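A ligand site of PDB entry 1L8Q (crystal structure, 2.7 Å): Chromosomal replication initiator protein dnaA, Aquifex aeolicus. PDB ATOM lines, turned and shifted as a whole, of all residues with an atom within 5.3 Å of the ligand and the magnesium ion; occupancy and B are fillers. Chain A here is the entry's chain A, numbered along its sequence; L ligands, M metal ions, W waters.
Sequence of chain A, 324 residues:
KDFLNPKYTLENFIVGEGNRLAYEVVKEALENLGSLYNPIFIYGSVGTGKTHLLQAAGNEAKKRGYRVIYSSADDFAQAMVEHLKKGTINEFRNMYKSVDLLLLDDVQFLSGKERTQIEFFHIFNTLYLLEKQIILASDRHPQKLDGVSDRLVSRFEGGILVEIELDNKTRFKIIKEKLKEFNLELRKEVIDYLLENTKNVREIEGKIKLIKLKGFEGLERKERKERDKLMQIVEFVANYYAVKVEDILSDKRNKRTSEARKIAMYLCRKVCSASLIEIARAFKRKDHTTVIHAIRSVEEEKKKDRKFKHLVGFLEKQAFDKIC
OG1 of Thr 51 sits close to OD2 of Asp 105 (2.6 Å).
A ring nitrogen (NE2) of His 52 is in hydrogen-bond range of the side-chain amide nitrogen (ND2) of Asn 12.
NZ of Lys 50 sits at hydrogen-bond distance from O of Ser 45.
The backbone carbonyl oxygen of Ile 14 sits close to the side-chain amide oxygen of Asn 19.
The backbone carbonyl oxygen (O) of Ser 45 sits close to the side-chain hydroxyl (OG1) of Thr 48, at 3.2 Å.
The backbone carbonyl oxygen (O) of Lys 7 lies close to the side-chain amide oxygen (OD1) of Asn 12 (3.1 Å).
N of Thr 51 sits at hydrogen-bond distance from O4 of the ligand (3.0 Å).
The backbone NH (N) of His 52 is in hydrogen-bond range of an oxygen (O4) of the ligand (2.6 Å).
A ring nitrogen (ND1) of His 52 lies within hydrogen-bond range of an oxygen (O10) of the ligand, at 2.6 Å.
The backbone NH of Lys 50 is in hydrogen-bond range of an oxygen (O2) of the ligand (3.1 Å).
The side-chain amino group of Lys 50 lies within salt-bridge range of an oxygen (O2) of the ligand (2.7 Å).
N of Ile 14 sits at hydrogen-bond distance from N4 of the ligand (3.0 Å).
The backbone carbonyl oxygen (O) of Ile 14 sits at hydrogen-bond distance from a nitrogen (N3) of the ligand.
An oxygen (O3) of the ligand lies within hydrogen-bond range of the backbone NH (N) of Gly 47 (2.7 Å).
An oxygen (O2) of the ligand is in hydrogen-bond range of the backbone NH (N) of Thr 48 (2.9 Å).
The backbone NH (N) of Gly 49 is in hydrogen-bond range of an oxygen (O2) of the ligand (3.2 Å).
N3 of the ligand is in hydrogen-bond range of OD1 of Asn 19, 3.4 Å away.
Merely in contact with the magnesium ion: Asp 105.
Within 4 Å of the magnesium ion: Thr 51 and Asp 105.
Water W3 lies within hydrogen-bond range of the side-chain carboxylate (OD1) of Asp 105 (2.8 Å) and the side-chain carboxylate (OD2) of Asp 106 (2.8 Å).
Water W6 lies within hydrogen-bond range of an oxygen (O8) of the ligand (2.6 Å), the backbone carbonyl oxygen (O) of Gly 47 (3.0 Å) and the backbone NH (N) of Val 201 (3.1 Å).
Water W7 lies within hydrogen-bond range of the side-chain hydroxyl (OH) of Tyr 8 (2.6 Å) and an oxygen (O5) of the ligand (2.7 Å).
Tyr 8 touches the ligand.
Asn 12 touches the ligand (O to C9, 3.6 Å).
Phe 13 touches the ligand.
Ser 45 touches the ligand (O to O2, 3.8 Å).
Val 46 touches the ligand.
Leu 166 touches the ligand.
CD1 of Ile 174 touches N5 of the ligand, at 3.6 Å.
Val 201 touches the ligand (CB to O8, 3.4 Å).
Within 4 Å of the ligand: Tyr 8, Asn 12, Phe 13, Ile 14, Asn 19, Ser 45, Val 46, Gly 47, Thr 48, Gly 49, Lys 50, Thr 51, His 52, Leu 166, Ile 174 and Val 201.
Along chain A the residues within 4 Å of the ligand span positions 8 to 201.
The nearest printed residue that does not touch the ligand is Thr 170 (4.1 Å).
The magnesium ion is bound by water W1 (1.8 Å), an oxygen (O1) of the ligand (1.9 Å), the side-chain hydroxyl of Thr 51 (2.0 Å), water W4 (2.1 Å), water W2 (2.2 Å) and water W3 (2.2 Å).
The magnesium ion has six donor atoms within binding distance.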
ATOM      1  N   LYS A   7      -3.087   2.947 -22.287  1.00  0.00           N
ATOM      2  CA  LYS A   7      -4.001   2.886 -23.436  1.00  0.00           C
ATOM      3  C   LYS A   7      -5.331   3.635 -23.264  1.00  0.00           C
ATOM      4  O   LYS A   7      -5.960   4.019 -24.233  1.00  0.00           O
ATOM      5  CB  LYS A   7      -4.258   1.436 -23.873  1.00  0.00           C
ATOM      6  CG  LYS A   7      -5.451   0.783 -23.188  1.00  0.00           C
ATOM      7  CD  LYS A   7      -5.595  -0.694 -23.589  1.00  0.00           C
ATOM      8  CE  LYS A   7      -6.734  -1.362 -22.803  1.00  0.00           C
ATOM      9  NZ  LYS A   7      -6.964  -2.790 -23.202  1.00  0.00           N
ATOM     10  N   TYR A   8      -5.758   3.840 -22.019  1.00  0.00           N
ATOM     11  CA  TYR A   8      -6.997   4.552 -21.749  1.00  0.00           C
ATOM     12  C   TYR A   8      -6.735   6.034 -21.626  1.00  0.00           C
ATOM     13  O   TYR A   8      -5.983   6.440 -20.739  1.00  0.00           O
ATOM     14  CB  TYR A   8      -7.595   4.092 -20.426  1.00  0.00           C
ATOM     15  CG  TYR A   8      -7.914   2.616 -20.302  1.00  0.00           C
ATOM     16  CD1 TYR A   8      -8.963   2.050 -21.024  1.00  0.00           C
ATOM     17  CD2 TYR A   8      -7.232   1.806 -19.401  1.00  0.00           C
ATOM     18  CE1 TYR A   8      -9.283   0.715 -20.872  1.00  0.00           C
ATOM     19  CE2 TYR A   8      -7.543   0.486 -19.249  1.00  0.00           C
ATOM     20  CZ  TYR A   8      -8.574  -0.063 -19.974  1.00  0.00           C
ATOM     21  OH  TYR A   8      -8.882  -1.392 -19.819  1.00  0.00           O
ATOM     22  N   ASN A  12      -8.986   9.458 -26.145  1.00  0.00           N
ATOM     23  CA  ASN A  12      -9.638   8.412 -26.926  1.00  0.00           C
ATOM     24  C   ASN A  12     -10.943   7.917 -26.317  1.00  0.00           C
ATOM     25  O   ASN A  12     -11.434   6.856 -26.673  1.00  0.00           O
ATOM     26  CB  ASN A  12      -8.704   7.243 -27.289  1.00  0.00           C
ATOM     27  CG  ASN A  12      -8.001   6.631 -26.076  1.00  0.00           C
ATOM     28  OD1 ASN A  12      -6.835   6.262 -26.169  1.00  0.00           O
ATOM     29  ND2 ASN A  12      -8.713   6.511 -24.948  1.00  0.00           N
ATOM     30  N   PHE A  13     -11.487   8.697 -25.390  1.00  0.00           N
ATOM     31  CA  PHE A  13     -12.811   8.419 -24.876  1.00  0.00           C
ATOM     32  C   PHE A  13     -13.783   9.133 -25.798  1.00  0.00           C
ATOM     33  O   PHE A  13     -13.747  10.363 -25.898  1.00  0.00           O
ATOM     34  CB  PHE A  13     -12.974   8.929 -23.450  1.00  0.00           C
ATOM     35  CG  PHE A  13     -14.240   8.465 -22.753  1.00  0.00           C
ATOM     36  CD1 PHE A  13     -14.290   7.246 -22.096  1.00  0.00           C
ATOM     37  CD2 PHE A  13     -15.381   9.269 -22.747  1.00  0.00           C
ATOM     38  CE1 PHE A  13     -15.448   6.833 -21.458  1.00  0.00           C
ATOM     39  CE2 PHE A  13     -16.535   8.860 -22.100  1.00  0.00           C
ATOM     40  CZ  PHE A  13     -16.567   7.644 -21.451  1.00  0.00           C
ATOM     41  N   ILE A  14     -14.600   8.372 -26.513  1.00  0.00           N
ATOM     42  CA  ILE A  14     -15.611   8.983 -27.370  1.00  0.00           C
ATOM     43  C   ILE A  14     -16.810   9.418 -26.536  1.00  0.00           C
ATOM     44  O   ILE A  14     -17.251   8.691 -25.650  1.00  0.00           O
ATOM     45  CB  ILE A  14     -16.026   8.009 -28.487  1.00  0.00           C
ATOM     46  CG1 ILE A  14     -14.794   7.485 -29.221  1.00  0.00           C
ATOM     47  CG2 ILE A  14     -16.968   8.701 -29.470  1.00  0.00           C
ATOM     48  CD1 ILE A  14     -15.111   6.567 -30.370  1.00  0.00           C
ATOM     49  N   VAL A  15     -17.327  10.594 -26.827  1.00  0.00           N
ATOM     50  CA  VAL A  15     -18.382  11.187 -26.034  1.00  0.00           C
ATOM     51  C   VAL A  15     -19.703  11.227 -26.785  1.00  0.00           C
ATOM     52  O   VAL A  15     -19.757  11.616 -27.941  1.00  0.00           O
ATOM     53  CB  VAL A  15     -17.978  12.610 -25.564  1.00  0.00           C
ATOM     54  CG1 VAL A  15     -19.099  13.259 -24.769  1.00  0.00           C
ATOM     55  CG2 VAL A  15     -16.674  12.540 -24.720  1.00  0.00           C
ATOM     56  N   ASN A  19     -22.643   9.311 -21.957  1.00  0.00           N
ATOM     57  CA  ASN A  19     -21.488   9.339 -21.061  1.00  0.00           C
ATOM     58  C   ASN A  19     -20.932  10.738 -20.857  1.00  0.00           C
ATOM     59  O   ASN A  19     -19.875  10.924 -20.255  1.00  0.00           O
ATOM     60  CB  ASN A  19     -20.388   8.395 -21.553  1.00  0.00           C
ATOM     61  CG  ASN A  19     -20.011   8.615 -23.037  1.00  0.00           C
ATOM     62  OD1 ASN A  19     -19.482   7.717 -23.700  1.00  0.00           O
ATOM     63  ND2 ASN A  19     -20.295   9.810 -23.554  1.00  0.00           N
ATOM     64  N   SER A  45     -23.552  -0.231 -16.247  1.00  0.00           N
ATOM     65  CA  SER A  45     -23.423  -1.652 -16.494  1.00  0.00           C
ATOM     66  C   SER A  45     -22.083  -1.975 -17.168  1.00  0.00           C
ATOM     67  O   SER A  45     -21.361  -1.068 -17.596  1.00  0.00           O
ATOM     68  CB  SER A  45     -24.557  -2.104 -17.388  1.00  0.00           C
ATOM     69  OG  SER A  45     -24.368  -1.565 -18.682  1.00  0.00           O
ATOM     70  N   VAL A  46     -21.784  -3.259 -17.279  1.00  0.00           N
ATOM     71  CA  VAL A  46     -20.523  -3.695 -17.879  1.00  0.00           C
ATOM     72  C   VAL A  46     -20.228  -3.128 -19.267  1.00  0.00           C
ATOM     73  O   VAL A  46     -21.104  -3.068 -20.121  1.00  0.00           O
ATOM     74  CB  VAL A  46     -20.440  -5.256 -17.932  1.00  0.00           C
ATOM     75  CG1 VAL A  46     -19.238  -5.683 -18.712  1.00  0.00           C
ATOM     76  CG2 VAL A  46     -20.332  -5.841 -16.517  1.00  0.00           C
ATOM     77  N   GLY A  47     -18.978  -2.747 -19.490  1.00  0.00           N
ATOM     78  CA  GLY A  47     -18.516  -2.306 -20.795  1.00  0.00           C
ATOM     79  C   GLY A  47     -19.108  -0.970 -21.130  1.00  0.00           C
ATOM     80  O   GLY A  47     -19.515  -0.723 -22.247  1.00  0.00           O
ATOM     81  N   THR A  48     -19.104  -0.087 -20.164  1.00  0.00           N
ATOM     82  CA  THR A  48     -19.813   1.146 -20.318  1.00  0.00           C
ATOM     83  C   THR A  48     -18.914   2.363 -20.220  1.00  0.00           C
ATOM     84  O   THR A  48     -19.364   3.486 -20.443  1.00  0.00           O
ATOM     85  CB  THR A  48     -20.912   1.161 -19.279  1.00  0.00           C
ATOM     86  OG1 THR A  48     -22.180   0.942 -19.930  1.00  0.00           O
ATOM     87  CG2 THR A  48     -21.041   2.522 -18.673  1.00  0.00           C
ATOM     88  N   GLY A  49     -17.643   2.132 -19.902  1.00  0.00           N
ATOM     89  CA  GLY A  49     -16.677   3.206 -19.836  1.00  0.00           C
ATOM     90  C   GLY A  49     -16.081   3.507 -18.466  1.00  0.00           C
ATOM     91  O   GLY A  49     -15.177   4.336 -18.340  1.00  0.00           O
ATOM     92  N   LYS A  50     -16.579   2.833 -17.426  1.00  0.00           N
ATOM     93  CA  LYS A  50     -16.116   3.096 -16.064  1.00  0.00           C
ATOM     94  C   LYS A  50     -14.595   2.963 -15.911  1.00  0.00           C
ATOM     95  O   LYS A  50     -13.926   3.907 -15.492  1.00  0.00           O
ATOM     96  CB  LYS A  50     -16.863   2.205 -15.054  1.00  0.00           C
ATOM     97  CG  LYS A  50     -18.380   2.330 -15.135  1.00  0.00           C
ATOM     98  CD  LYS A  50     -19.103   1.437 -14.122  1.00  0.00           C
ATOM     99  CE  LYS A  50     -18.597   0.005 -14.191  1.00  0.00           C
ATOM    100  NZ  LYS A  50     -19.059  -0.741 -15.407  1.00  0.00           N
ATOM    101  N   THR A  51     -14.038   1.820 -16.269  1.00  0.00           N
ATOM    102  CA  THR A  51     -12.622   1.614 -16.059  1.00  0.00           C
ATOM    103  C   THR A  51     -11.820   2.545 -16.970  1.00  0.00           C
ATOM    104  O   THR A  51     -10.850   3.182 -16.556  1.00  0.00           O
ATOM    105  CB  THR A  51     -12.251   0.148 -16.292  1.00  0.00           C
ATOM    106  OG1 THR A  51     -12.895  -0.669 -15.301  1.00  0.00           O
ATOM    107  CG2 THR A  51     -10.753  -0.087 -16.021  1.00  0.00           C
ATOM    108  N   HIS A  52     -12.248   2.648 -18.200  1.00  0.00           N
ATOM    109  CA  HIS A  52     -11.584   3.512 -19.138  1.00  0.00           C
ATOM    110  C   HIS A  52     -11.501   4.940 -18.582  1.00  0.00           C
ATOM    111  O   HIS A  52     -10.447   5.577 -18.631  1.00  0.00           O
ATOM    112  CB  HIS A  52     -12.350   3.492 -20.452  1.00  0.00           C
ATOM    113  CG  HIS A  52     -11.693   4.295 -21.536  1.00  0.00           C
ATOM    114  ND1 HIS A  52     -11.442   3.771 -22.792  1.00  0.00           N
ATOM    115  CD2 HIS A  52     -11.224   5.559 -21.552  1.00  0.00           C
ATOM    116  CE1 HIS A  52     -10.869   4.691 -23.529  1.00  0.00           C
ATOM    117  NE2 HIS A  52     -10.721   5.787 -22.808  1.00  0.00           N
ATOM    118  N   LEU A  53     -12.613   5.445 -18.067  1.00  0.00           N
ATOM    119  CA  LEU A  53     -12.669   6.802 -17.584  1.00  0.00           C
ATOM    120  C   LEU A  53     -11.796   7.004 -16.332  1.00  0.00           C
ATOM    121  O   LEU A  53     -11.088   8.006 -16.217  1.00  0.00           O
ATOM    122  CB  LEU A  53     -14.117   7.208 -17.318  1.00  0.00           C
ATOM    123  CG  LEU A  53     -14.479   8.668 -17.181  1.00  0.00           C
ATOM    124  CD1 LEU A  53     -13.998   9.452 -18.372  1.00  0.00           C
ATOM    125  CD2 LEU A  53     -15.985   8.772 -17.067  1.00  0.00           C
ATOM    126  N   ASP A 105     -11.968   1.115  -8.328  1.00  0.00           N
ATOM    127  CA  ASP A 105     -12.850   0.608  -9.350  1.00  0.00           C
ATOM    128  C   ASP A 105     -13.638  -0.586  -8.818  1.00  0.00           C
ATOM    129  O   ASP A 105     -13.137  -1.311  -7.976  1.00  0.00           O
ATOM    130  CB  ASP A 105     -11.998   0.156 -10.515  1.00  0.00           C
ATOM    131  CG  ASP A 105     -12.743   0.144 -11.829  1.00  0.00           C
ATOM    132  OD1 ASP A 105     -13.969   0.388 -11.853  1.00  0.00           O
ATOM    133  OD2 ASP A 105     -12.162  -0.088 -12.913  1.00  0.00           O
ATOM    134  N   ASP A 106     -14.863  -0.783  -9.309  1.00  0.00           N
ATOM    135  CA  ASP A 106     -15.698  -1.917  -8.916  1.00  0.00           C
ATOM    136  C   ASP A 106     -16.048  -2.019  -7.404  1.00  0.00           C
ATOM    137  O   ASP A 106     -16.014  -3.115  -6.829  1.00  0.00           O
ATOM    138  CB  ASP A 106     -15.099  -3.221  -9.404  1.00  0.00           C
ATOM    139  CG  ASP A 106     -15.097  -3.322 -10.933  1.00  0.00           C
ATOM    140  OD1 ASP A 106     -14.155  -3.956 -11.494  1.00  0.00           O
ATOM    141  OD2 ASP A 106     -15.971  -2.813 -11.669  1.00  0.00           O
ATOM    142  N   LEU A 166     -23.434   3.436 -22.524  1.00  0.00           N
ATOM    143  CA  LEU A 166     -22.860   3.377 -23.852  1.00  0.00           C
ATOM    144  C   LEU A 166     -23.993   3.377 -24.854  1.00  0.00           C
ATOM    145  O   LEU A 166     -24.542   2.337 -25.183  1.00  0.00           O
ATOM    146  CB  LEU A 166     -22.035   2.126 -24.011  1.00  0.00           C
ATOM    147  CG  LEU A 166     -21.060   2.191 -25.178  1.00  0.00           C
ATOM    148  CD1 LEU A 166     -19.879   3.044 -24.766  1.00  0.00           C
ATOM    149  CD2 LEU A 166     -20.595   0.815 -25.575  1.00  0.00           C
ATOM    150  N   THR A 170     -22.771   6.233 -29.803  1.00  0.00           N
ATOM    151  CA  THR A 170     -21.412   5.990 -29.339  1.00  0.00           C
ATOM    152  C   THR A 170     -20.832   4.644 -29.835  1.00  0.00           C
ATOM    153  O   THR A 170     -19.737   4.605 -30.398  1.00  0.00           O
ATOM    154  CB  THR A 170     -21.345   6.136 -27.813  1.00  0.00           C
ATOM    155  OG1 THR A 170     -21.557   7.514 -27.476  1.00  0.00           O
ATOM    156  CG2 THR A 170     -19.957   5.878 -27.295  1.00  0.00           C
ATOM    157  N   ILE A 174     -17.546   3.845 -32.055  1.00  0.00           N
ATOM    158  CA  ILE A 174     -16.564   2.870 -31.606  1.00  0.00           C
ATOM    159  C   ILE A 174     -16.413   1.773 -32.679  1.00  0.00           C
ATOM    160  O   ILE A 174     -15.295   1.467 -33.137  1.00  0.00           O
ATOM    161  CB  ILE A 174     -16.964   2.290 -30.250  1.00  0.00           C
ATOM    162  CG1 ILE A 174     -16.746   3.342 -29.159  1.00  0.00           C
ATOM    163  CG2 ILE A 174     -16.134   1.071 -29.941  1.00  0.00           C
ATOM    164  CD1 ILE A 174     -17.154   2.887 -27.752  1.00  0.00           C
ATOM    165  N   GLU A 177     -14.159   2.763 -35.250  1.00  0.00           N
ATOM    166  CA  GLU A 177     -12.756   2.734 -34.823  1.00  0.00           C
ATOM    167  C   GLU A 177     -12.235   1.303 -34.839  1.00  0.00           C
ATOM    168  O   GLU A 177     -11.179   1.048 -35.378  1.00  0.00           O
ATOM    169  CB  GLU A 177     -12.521   3.449 -33.460  1.00  0.00           C
ATOM    170  CG  GLU A 177     -11.988   4.894 -33.600  1.00  0.00           C
ATOM    171  CD  GLU A 177     -12.110   5.752 -32.308  1.00  0.00           C
ATOM    172  OE1 GLU A 177     -11.874   5.229 -31.177  1.00  0.00           O
ATOM    173  OE2 GLU A 177     -12.427   6.974 -32.433  1.00  0.00           O
ATOM    174  N   VAL A 201     -17.703  -3.500 -26.212  1.00  0.00           N
ATOM    175  CA  VAL A 201     -16.593  -3.579 -27.118  1.00  0.00           C
ATOM    176  C   VAL A 201     -16.132  -5.040 -27.130  1.00  0.00           C
ATOM    177  O   VAL A 201     -15.579  -5.520 -28.132  1.00  0.00           O
ATOM    178  CB  VAL A 201     -15.427  -2.680 -26.652  1.00  0.00           C
ATOM    179  CG1 VAL A 201     -14.094  -3.333 -26.941  1.00  0.00           C
ATOM    180  CG2 VAL A 201     -15.510  -1.347 -27.330  1.00  0.00           C
HETATM  181  P1  LIG L   1     -16.460  -1.014 -17.834  1.00  0.00           P
HETATM  182  O1  LIG L   1     -15.247  -0.673 -16.957  1.00  0.00           O
HETATM  183  O2  LIG L   1     -17.647  -0.112 -17.617  1.00  0.00           O
HETATM  184  O3  LIG L   1     -16.784  -2.477 -17.869  1.00  0.00           O
HETATM  185  P2  LIG L   1     -14.505  -0.388 -19.645  1.00  0.00           P
HETATM  186  O4  LIG L   1     -14.045   0.969 -19.132  1.00  0.00           O
HETATM  187  O5  LIG L   1     -13.694  -1.545 -19.061  1.00  0.00           O
HETATM  188  O6  LIG L   1     -16.036  -0.653 -19.310  1.00  0.00           O
HETATM  189  O7  LIG L   1     -14.472  -0.401 -21.240  1.00  0.00           O
HETATM  190  C1  LIG L   1     -14.768  -1.588 -21.951  1.00  0.00           C
HETATM  191  C2  LIG L   1     -14.102  -1.431 -23.290  1.00  0.00           C
HETATM  192  O8  LIG L   1     -14.857  -0.525 -24.122  1.00  0.00           O
HETATM  193  C3  LIG L   1     -12.738  -0.789 -23.105  1.00  0.00           C
HETATM  194  O9  LIG L   1     -11.926  -1.334 -24.138  1.00  0.00           O
HETATM  195  C4  LIG L   1     -13.015   0.671 -23.360  1.00  0.00           C
HETATM  196  O10 LIG L   1     -11.904   1.448 -23.783  1.00  0.00           O
HETATM  197  C5  LIG L   1     -14.083   0.641 -24.422  1.00  0.00           C
HETATM  198  N1  LIG L   1     -14.890   1.854 -24.263  1.00  0.00           N
HETATM  199  C6  LIG L   1     -15.846   2.065 -23.320  1.00  0.00           C
HETATM  200  N2  LIG L   1     -16.384   3.314 -23.470  1.00  0.00           N
HETATM  201  C7  LIG L   1     -15.758   3.906 -24.489  1.00  0.00           C
HETATM  202  C8  LIG L   1     -15.836   5.207 -25.167  1.00  0.00           C
HETATM  203  N3  LIG L   1     -16.704   6.154 -24.775  1.00  0.00           N
HETATM  204  N4  LIG L   1     -15.003   5.435 -26.196  1.00  0.00           N
HETATM  205  C9  LIG L   1     -14.131   4.501 -26.620  1.00  0.00           C
HETATM  206  N5  LIG L   1     -14.010   3.290 -26.050  1.00  0.00           N
HETATM  207  C10 LIG L   1     -14.784   2.954 -25.007  1.00  0.00           C
HETATM  208 MG    MG M   1     -14.433  -1.794 -15.728  1.00  0.00          MG
HETATM  209  O   HOH W   1     -13.787  -2.968 -16.950  1.00  0.00           O
HETATM  210  O   HOH W   2     -15.992  -3.289 -15.569  1.00  0.00           O
HETATM  211  O   HOH W   3     -15.266  -1.110 -13.840  1.00  0.00           O
HETATM  212  O   HOH W   4     -13.672  -3.090 -14.264  1.00  0.00           O
HETATM  213  O   HOH W   5     -15.453  -4.521 -19.123  1.00  0.00           O
HETATM  214  O   HOH W   6     -17.395  -1.061 -24.299  1.00  0.00           O
HETATM  215  O   HOH W   7     -11.384  -2.084 -20.339  1.00  0.00           O
